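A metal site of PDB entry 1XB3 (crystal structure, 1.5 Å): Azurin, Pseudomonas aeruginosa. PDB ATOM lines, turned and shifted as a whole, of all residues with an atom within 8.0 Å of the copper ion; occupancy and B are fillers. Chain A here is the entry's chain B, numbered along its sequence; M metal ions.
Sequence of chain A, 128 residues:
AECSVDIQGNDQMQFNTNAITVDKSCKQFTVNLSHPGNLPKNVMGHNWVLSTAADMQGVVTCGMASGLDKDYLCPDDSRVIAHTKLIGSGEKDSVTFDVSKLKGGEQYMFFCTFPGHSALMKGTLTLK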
ATOM      1  N   GLY A   9       2.049   6.881  25.292  1.00  0.00           N
ATOM      2  CA  GLY A   9       3.176   6.725  24.351  1.00  0.00           C
ATOM      3  C   GLY A   9       4.345   6.271  25.211  1.00  0.00           C
ATOM      4  O   GLY A   9       4.596   6.817  26.267  1.00  0.00           O
ATOM      5  N   ASN A  10       5.111   5.275  24.736  1.00  0.00           N
ATOM      6  CA  ASN A  10       6.123   4.658  25.574  1.00  0.00           C
ATOM      7  C   ASN A  10       7.514   4.865  25.015  1.00  0.00           C
ATOM      8  O   ASN A  10       7.699   5.576  24.009  1.00  0.00           O
ATOM      9  CB  ASN A  10       5.780   3.183  25.853  1.00  0.00           C
ATOM     10  CG  ASN A  10       5.972   2.294  24.673  1.00  0.00           C
ATOM     11  OD1 ASN A  10       6.513   2.719  23.662  1.00  0.00           O
ATOM     12  ND2 ASN A  10       5.509   1.053  24.763  1.00  0.00           N
ATOM     13  N   MET A  13       8.483   3.740  21.150  1.00  0.00           N
ATOM     14  CA  MET A  13       7.861   4.388  20.015  1.00  0.00           C
ATOM     15  C   MET A  13       6.520   3.770  19.652  1.00  0.00           C
ATOM     16  O   MET A  13       6.213   3.630  18.467  1.00  0.00           O
ATOM     17  CB  MET A  13       8.789   4.322  18.785  1.00  0.00           C
ATOM     18  CG  MET A  13       8.548   5.409  17.756  1.00  0.00           C
ATOM     19  SD  MET A  13       9.686   5.383  16.363  1.00  0.00           S
ATOM     20  CE  MET A  13      11.189   5.798  17.165  1.00  0.00           C
ATOM     21  N   GLN A  14       5.711   3.430  20.678  1.00  0.00           N
ATOM     22  CA  GLN A  14       4.357   2.938  20.414  1.00  0.00           C
ATOM     23  C   GLN A  14       3.337   3.674  21.242  1.00  0.00           C
ATOM     24  O   GLN A  14       3.597   4.024  22.406  1.00  0.00           O
ATOM     25  CB  GLN A  14       4.169   1.456  20.714  1.00  0.00           C
ATOM     26  CG  GLN A  14       5.092   0.518  19.926  1.00  0.00           C
ATOM     27  CD  GLN A  14       4.575   0.123  18.553  1.00  0.00           C
ATOM     28  OE1 GLN A  14       3.408   0.372  18.197  1.00  0.00           O
ATOM     29  NE2 GLN A  14       5.445  -0.504  17.766  1.00  0.00           N
ATOM     30  N   PHE A  15       2.174   3.889  20.641  1.00  0.00           N
ATOM     31  CA  PHE A  15       0.959   4.178  21.405  1.00  0.00           C
ATOM     32  C   PHE A  15       0.369   2.840  21.849  1.00  0.00           C
ATOM     33  O   PHE A  15       0.599   1.810  21.182  1.00  0.00           O
ATOM     34  CB  PHE A  15      -0.058   4.885  20.553  1.00  0.00           C
ATOM     35  CG  PHE A  15       0.185   6.352  20.338  1.00  0.00           C
ATOM     36  CD1 PHE A  15       0.087   6.878  19.071  1.00  0.00           C
ATOM     37  CD2 PHE A  15       0.430   7.221  21.411  1.00  0.00           C
ATOM     38  CE1 PHE A  15       0.232   8.230  18.825  1.00  0.00           C
ATOM     39  CE2 PHE A  15       0.609   8.596  21.167  1.00  0.00           C
ATOM     40  CZ  PHE A  15       0.473   9.082  19.898  1.00  0.00           C
ATOM     41  N   LEU A  33      -3.301  11.876  27.556  1.00  0.00           N
ATOM     42  CA  LEU A  33      -2.042  11.321  27.087  1.00  0.00           C
ATOM     43  C   LEU A  33      -1.049  11.262  28.219  1.00  0.00           C
ATOM     44  O   LEU A  33      -0.874  12.229  28.960  1.00  0.00           O
ATOM     45  CB  LEU A  33      -1.448  12.195  25.978  1.00  0.00           C
ATOM     46  CG  LEU A  33      -0.105  11.713  25.385  1.00  0.00           C
ATOM     47  CD1 LEU A  33      -0.309  10.420  24.590  1.00  0.00           C
ATOM     48  CD2 LEU A  33       0.522  12.734  24.481  1.00  0.00           C
ATOM     49  N   HIS A  35       3.041   9.390  29.306  1.00  0.00           N
ATOM     50  CA  HIS A  35       4.275   8.826  28.767  1.00  0.00           C
ATOM     51  C   HIS A  35       5.041   8.133  29.904  1.00  0.00           C
ATOM     52  O   HIS A  35       5.913   8.758  30.490  1.00  0.00           O
ATOM     53  CB  HIS A  35       5.109   9.955  28.164  1.00  0.00           C
ATOM     54  CG  HIS A  35       6.383   9.501  27.526  1.00  0.00           C
ATOM     55  ND1 HIS A  35       7.095  10.292  26.659  1.00  0.00           N
ATOM     56  CD2 HIS A  35       7.078   8.344  27.634  1.00  0.00           C
ATOM     57  CE1 HIS A  35       8.195   9.644  26.285  1.00  0.00           C
ATOM     58  NE2 HIS A  35       8.210   8.466  26.858  1.00  0.00           N
ATOM     59  N   LYS A  41      12.032  14.230  26.657  1.00  0.00           N
ATOM     60  CA  LYS A  41      11.309  14.750  25.534  1.00  0.00           C
ATOM     61  C   LYS A  41      12.155  15.011  24.298  1.00  0.00           C
ATOM     62  O   LYS A  41      11.661  14.864  23.165  1.00  0.00           O
ATOM     63  CB  LYS A  41      10.623  16.037  26.009  1.00  0.00           C
ATOM     64  CG  LYS A  41       9.616  16.601  25.056  1.00  0.00           C
ATOM     65  CD  LYS A  41       9.228  17.979  25.519  1.00  0.00           C
ATOM     66  CE  LYS A  41      10.348  18.988  25.231  1.00  0.00           C
ATOM     67  NZ  LYS A  41       9.959  20.389  25.606  1.00  0.00           N
ATOM     68  N   VAL A  43      14.519  13.299  22.978  1.00  0.00           N
ATOM     69  CA  VAL A  43      14.816  12.116  22.179  1.00  0.00           C
ATOM     70  C   VAL A  43      13.622  11.149  21.966  1.00  0.00           C
ATOM     71  O   VAL A  43      13.673  10.257  21.117  1.00  0.00           O
ATOM     72  CB  VAL A  43      15.959  11.291  22.811  1.00  0.00           C
ATOM     73  CG1 VAL A  43      17.231  12.111  22.974  1.00  0.00           C
ATOM     74  CG2 VAL A  43      15.547  10.624  24.137  1.00  0.00           C
ATOM     75  N   MET A  44      12.586  11.289  22.782  1.00  0.00           N
ATOM     76  CA  MET A  44      11.445  10.356  22.712  1.00  0.00           C
ATOM     77  C   MET A  44      10.155  11.093  23.104  1.00  0.00           C
ATOM     78  O   MET A  44       9.223  10.514  23.671  1.00  0.00           O
ATOM     79  CB  MET A  44      11.691   9.149  23.662  1.00  0.00           C
ATOM     80  CG  MET A  44      10.689   7.994  23.532  1.00  0.00           C
ATOM     81  SD  MET A  44      10.553   7.248  21.876  1.00  0.00           S
ATOM     82  CE  MET A  44      12.116   6.361  21.774  1.00  0.00           C
ATOM     83  N   GLY A  45      10.063  12.382  22.791  1.00  0.00           N
ATOM     84  CA  GLY A  45       8.843  13.133  23.089  1.00  0.00           C
ATOM     85  C   GLY A  45       7.670  12.637  22.280  1.00  0.00           C
ATOM     86  O   GLY A  45       7.839  12.199  21.137  1.00  0.00           O
ATOM     87  N   HIS A  46       6.482  12.707  22.872  1.00  0.00           N
ATOM     88  CA  HIS A  46       5.258  12.301  22.205  1.00  0.00           C
ATOM     89  C   HIS A  46       4.186  13.338  22.367  1.00  0.00           C
ATOM     90  O   HIS A  46       3.993  13.915  23.433  1.00  0.00           O
ATOM     91  CB  HIS A  46       4.698  11.000  22.743  1.00  0.00           C
ATOM     92  CG  HIS A  46       5.635   9.835  22.694  1.00  0.00           C
ATOM     93  ND1 HIS A  46       6.344   9.464  21.557  1.00  0.00           N
ATOM     94  CD2 HIS A  46       5.935   8.923  23.653  1.00  0.00           C
ATOM     95  CE1 HIS A  46       7.053   8.382  21.850  1.00  0.00           C
ATOM     96  NE2 HIS A  46       6.815   8.033  23.103  1.00  0.00           N
ATOM     97  N   ASN A  47       3.469  13.567  21.255  1.00  0.00           N
ATOM     98  CA  ASN A  47       2.207  14.305  21.320  1.00  0.00           C
ATOM     99  C   ASN A  47       1.083  13.499  20.727  1.00  0.00           C
ATOM    100  O   ASN A  47       1.335  12.411  20.180  1.00  0.00           O
ATOM    101  CB  ASN A  47       2.302  15.701  20.666  1.00  0.00           C
ATOM    102  CG  ASN A  47       2.816  15.671  19.258  1.00  0.00           C
ATOM    103  OD1 ASN A  47       2.845  14.618  18.634  1.00  0.00           O
ATOM    104  ND2 ASN A  47       3.215  16.855  18.726  1.00  0.00           N
ATOM    105  N   TRP A  48      -0.145  13.995  20.882  1.00  0.00           N
ATOM    106  CA  TRP A  48      -1.313  13.400  20.253  1.00  0.00           C
ATOM    107  C   TRP A  48      -1.940  14.497  19.421  1.00  0.00           C
ATOM    108  O   TRP A  48      -2.327  15.517  19.958  1.00  0.00           O
ATOM    109  CB  TRP A  48      -2.250  12.806  21.319  1.00  0.00           C
ATOM    110  CG  TRP A  48      -3.430  12.073  20.773  1.00  0.00           C
ATOM    111  CD1 TRP A  48      -3.525  10.760  20.573  1.00  0.00           C
ATOM    112  CD2 TRP A  48      -4.693  12.638  20.350  1.00  0.00           C
ATOM    113  NE1 TRP A  48      -4.778  10.420  20.103  1.00  0.00           N
ATOM    114  CE2 TRP A  48      -5.493  11.568  19.897  1.00  0.00           C
ATOM    115  CE3 TRP A  48      -5.217  13.930  20.303  1.00  0.00           C
ATOM    116  CZ2 TRP A  48      -6.792  11.762  19.395  1.00  0.00           C
ATOM    117  CZ3 TRP A  48      -6.525  14.120  19.799  1.00  0.00           C
ATOM    118  CH2 TRP A  48      -7.290  13.036  19.368  1.00  0.00           C
ATOM    119  N   LEU A  86       3.826  18.283  23.481  1.00  0.00           N
ATOM    120  CA  LEU A  86       4.815  17.232  23.417  1.00  0.00           C
ATOM    121  C   LEU A  86       5.301  16.942  24.824  1.00  0.00           C
ATOM    122  O   LEU A  86       5.696  17.856  25.547  1.00  0.00           O
ATOM    123  CB  LEU A  86       5.987  17.699  22.560  1.00  0.00           C
ATOM    124  CG  LEU A  86       7.004  16.673  22.082  1.00  0.00           C
ATOM    125  CD1 LEU A  86       6.427  15.853  20.936  1.00  0.00           C
ATOM    126  CD2 LEU A  86       8.268  17.369  21.640  1.00  0.00           C
ATOM    127  N   ILE A  87       5.294  15.669  25.195  1.00  0.00           N
ATOM    128  CA  ILE A  87       5.667  15.279  26.561  1.00  0.00           C
ATOM    129  C   ILE A  87       6.782  14.246  26.597  1.00  0.00           C
ATOM    130  O   ILE A  87       6.848  13.332  25.780  1.00  0.00           O
ATOM    131  CB  ILE A  87       4.456  14.759  27.350  1.00  0.00           C
ATOM    132  CG1 ILE A  87       3.832  13.512  26.723  1.00  0.00           C
ATOM    133  CG2 ILE A  87       3.417  15.889  27.521  1.00  0.00           C
ATOM    134  CD1 ILE A  87       2.752  12.886  27.598  1.00  0.00           C
ATOM    135  N   PHE A 111      -1.928  10.923  15.649  1.00  0.00           N
ATOM    136  CA  PHE A 111      -0.511  10.653  15.444  1.00  0.00           C
ATOM    137  C   PHE A 111       0.375  11.523  16.312  1.00  0.00           C
ATOM    138  O   PHE A 111      -0.054  12.564  16.848  1.00  0.00           O
ATOM    139  CB  PHE A 111      -0.117  10.827  13.955  1.00  0.00           C
ATOM    140  CG  PHE A 111      -0.589  12.087  13.348  1.00  0.00           C
ATOM    141  CD1 PHE A 111      -1.860  12.149  12.792  1.00  0.00           C
ATOM    142  CD2 PHE A 111       0.179  13.257  13.397  1.00  0.00           C
ATOM    143  CE1 PHE A 111      -2.350  13.355  12.274  1.00  0.00           C
ATOM    144  CE2 PHE A 111      -0.311  14.432  12.892  1.00  0.00           C
ATOM    145  CZ  PHE A 111      -1.601  14.486  12.333  1.00  0.00           C
ATOM    146  N   CYS A 112       1.621  11.053  16.472  1.00  0.00           N
ATOM    147  CA  CYS A 112       2.682  11.823  17.073  1.00  0.00           C
ATOM    148  C   CYS A 112       3.531  12.454  15.973  1.00  0.00           C
ATOM    149  O   CYS A 112       3.874  11.766  15.010  1.00  0.00           O
ATOM    150  CB  CYS A 112       3.534  10.949  17.994  1.00  0.00           C
ATOM    151  SG  CYS A 112       4.964  11.780  18.677  1.00  0.00           S
ATOM    152  N   THR A 113       3.908  13.739  16.126  1.00  0.00           N
ATOM    153  CA  THR A 113       4.695  14.428  15.129  1.00  0.00           C
ATOM    154  C   THR A 113       6.190  14.507  15.461  1.00  0.00           C
ATOM    155  O   THR A 113       6.952  15.105  14.711  1.00  0.00           O
ATOM    156  CB  THR A 113       4.184  15.830  14.855  1.00  0.00           C
ATOM    157  OG1 THR A 113       4.278  16.635  16.032  1.00  0.00           O
ATOM    158  CG2 THR A 113       2.775  15.771  14.405  1.00  0.00           C
ATOM    159  N   PHE A 114       6.631  13.878  16.563  1.00  0.00           N
ATOM    160  CA  PHE A 114       8.091  13.826  16.813  1.00  0.00           C
ATOM    161  C   PHE A 114       8.740  13.142  15.585  1.00  0.00           C
ATOM    162  O   PHE A 114       8.208  12.134  15.112  1.00  0.00           O
ATOM    163  CB  PHE A 114       8.387  13.072  18.113  1.00  0.00           C
ATOM    164  CG  PHE A 114       9.827  13.134  18.520  1.00  0.00           C
ATOM    165  CD1 PHE A 114      10.244  14.024  19.487  1.00  0.00           C
ATOM    166  CD2 PHE A 114      10.762  12.311  17.939  1.00  0.00           C
ATOM    167  CE1 PHE A 114      11.592  14.111  19.851  1.00  0.00           C
ATOM    168  CE2 PHE A 114      12.119  12.386  18.291  1.00  0.00           C
ATOM    169  CZ  PHE A 114      12.505  13.270  19.259  1.00  0.00           C
ATOM    170  N   PRO A 115       9.895  13.646  15.073  1.00  0.00           N
ATOM    171  CA  PRO A 115      10.463  13.082  13.858  1.00  0.00           C
ATOM    172  C   PRO A 115      10.583  11.577  13.841  1.00  0.00           C
ATOM    173  O   PRO A 115      11.194  10.974  14.735  1.00  0.00           O
ATOM    174  CB  PRO A 115      11.868  13.687  13.822  1.00  0.00           C
ATOM    175  CG  PRO A 115      11.642  15.029  14.386  1.00  0.00           C
ATOM    176  CD  PRO A 115      10.674  14.807  15.530  1.00  0.00           C
ATOM    177  N   GLY A 116       9.972  10.962  12.827  1.00  0.00           N
ATOM    178  CA  GLY A 116      10.038   9.529  12.655  1.00  0.00           C
ATOM    179  C   GLY A 116       8.954   8.724  13.359  1.00  0.00           C
ATOM    180  O   GLY A 116       8.651   7.598  12.958  1.00  0.00           O
ATOM    181  N   HIS A 117       8.357   9.278  14.423  1.00  0.00           N
ATOM    182  CA  HIS A 117       7.458   8.509  15.234  1.00  0.00           C
ATOM    183  C   HIS A 117       6.169   8.058  14.552  1.00  0.00           C
ATOM    184  O   HIS A 117       5.662   6.988  14.881  1.00  0.00           O
ATOM    185  CB  HIS A 117       7.089   9.229  16.539  1.00  0.00           C
ATOM    186  CG  HIS A 117       8.191   9.239  17.551  1.00  0.00           C
ATOM    187  ND1 HIS A 117       7.983   9.634  18.851  1.00  0.00           N
ATOM    188  CD2 HIS A 117       9.489   8.885  17.442  1.00  0.00           C
ATOM    189  CE1 HIS A 117       9.139   9.560  19.496  1.00  0.00           C
ATOM    190  NE2 HIS A 117      10.074   9.134  18.661  1.00  0.00           N
ATOM    191  N   SER A 118       5.639   8.858  13.642  1.00  0.00           N
ATOM    192  CA  SER A 118       4.295   8.586  13.088  1.00  0.00           C
ATOM    193  C   SER A 118       4.248   7.312  12.255  1.00  0.00           C
ATOM    194  O   SER A 118       3.142   6.833  11.960  1.00  0.00           O
ATOM    195  CB  SER A 118       3.743   9.732  12.272  1.00  0.00           C
ATOM    196  OG  SER A 118       4.422   9.897  11.034  1.00  0.00           O
ATOM    197  N   MET A 121       3.492   5.456  15.458  1.00  0.00           N
ATOM    198  CA  MET A 121       2.647   6.157  16.425  1.00  0.00           C
ATOM    199  C   MET A 121       1.530   6.893  15.711  1.00  0.00           C
ATOM    200  O   MET A 121       1.547   8.124  15.530  1.00  0.00           O
ATOM    201  CB  MET A 121       3.490   7.057  17.327  1.00  0.00           C
ATOM    202  CG  MET A 121       4.514   6.290  18.071  1.00  0.00           C
ATOM    203  SD  MET A 121       5.306   7.255  19.361  1.00  0.00           S
ATOM    204  CE  MET A 121       3.935   7.362  20.530  1.00  0.00           C
HETATM  205 CU    CU M   1       6.297  10.343  19.705  1.00  0.00          CU
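ND1 of His 117 lies close to O of Gly 45 (3.4 Å).
A ring nitrogen (NE2) of His 46 is in hydrogen-bond range of the backbone carbonyl oxygen (O) of Asn 10, at 2.8 Å.
ND1 of His 117 sits close to SD of Met 121 (3.6 Å).
A ring nitrogen (NE2) of His 117 sits close to the side-chain sulfur of Met 44 (3.8 Å).
The backbone carbonyl oxygen (O) of His 46 is in hydrogen-bond range of the backbone NH (N) of Ile 87, at 2.8 Å.
A ring nitrogen (ND1) of His 46 sits close to the side-chain sulfur of Met 121 (3.3 Å).
N of Cys 112 sits at hydrogen-bond distance from O of Met 121 (3.1 Å).
The side-chain sulfur (SG) of Cys 112 lies close to the backbone NH (N) of Phe 114.
CB of Phe 114 touches the copper ion, 3.8 Å away.
Met 121 touches the copper ion (SD to CU, 3.3 Å).
Along chain A the residues within 4 Å of the copper ion span positions 45 to 121.
The nearest printed residue that does not touch the copper ion is Asn 47 (4.6 Å).
The copper ion is bound by ND1 of His 117, at 2.0 Å.
ND1 of His 46 is bound to the copper ion (2.1 Å).
The copper ion is bound by SG of Cys 112 (2.2 Å).
Slightly farther from the copper ion lies O of Gly 45 (2.8 Å).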
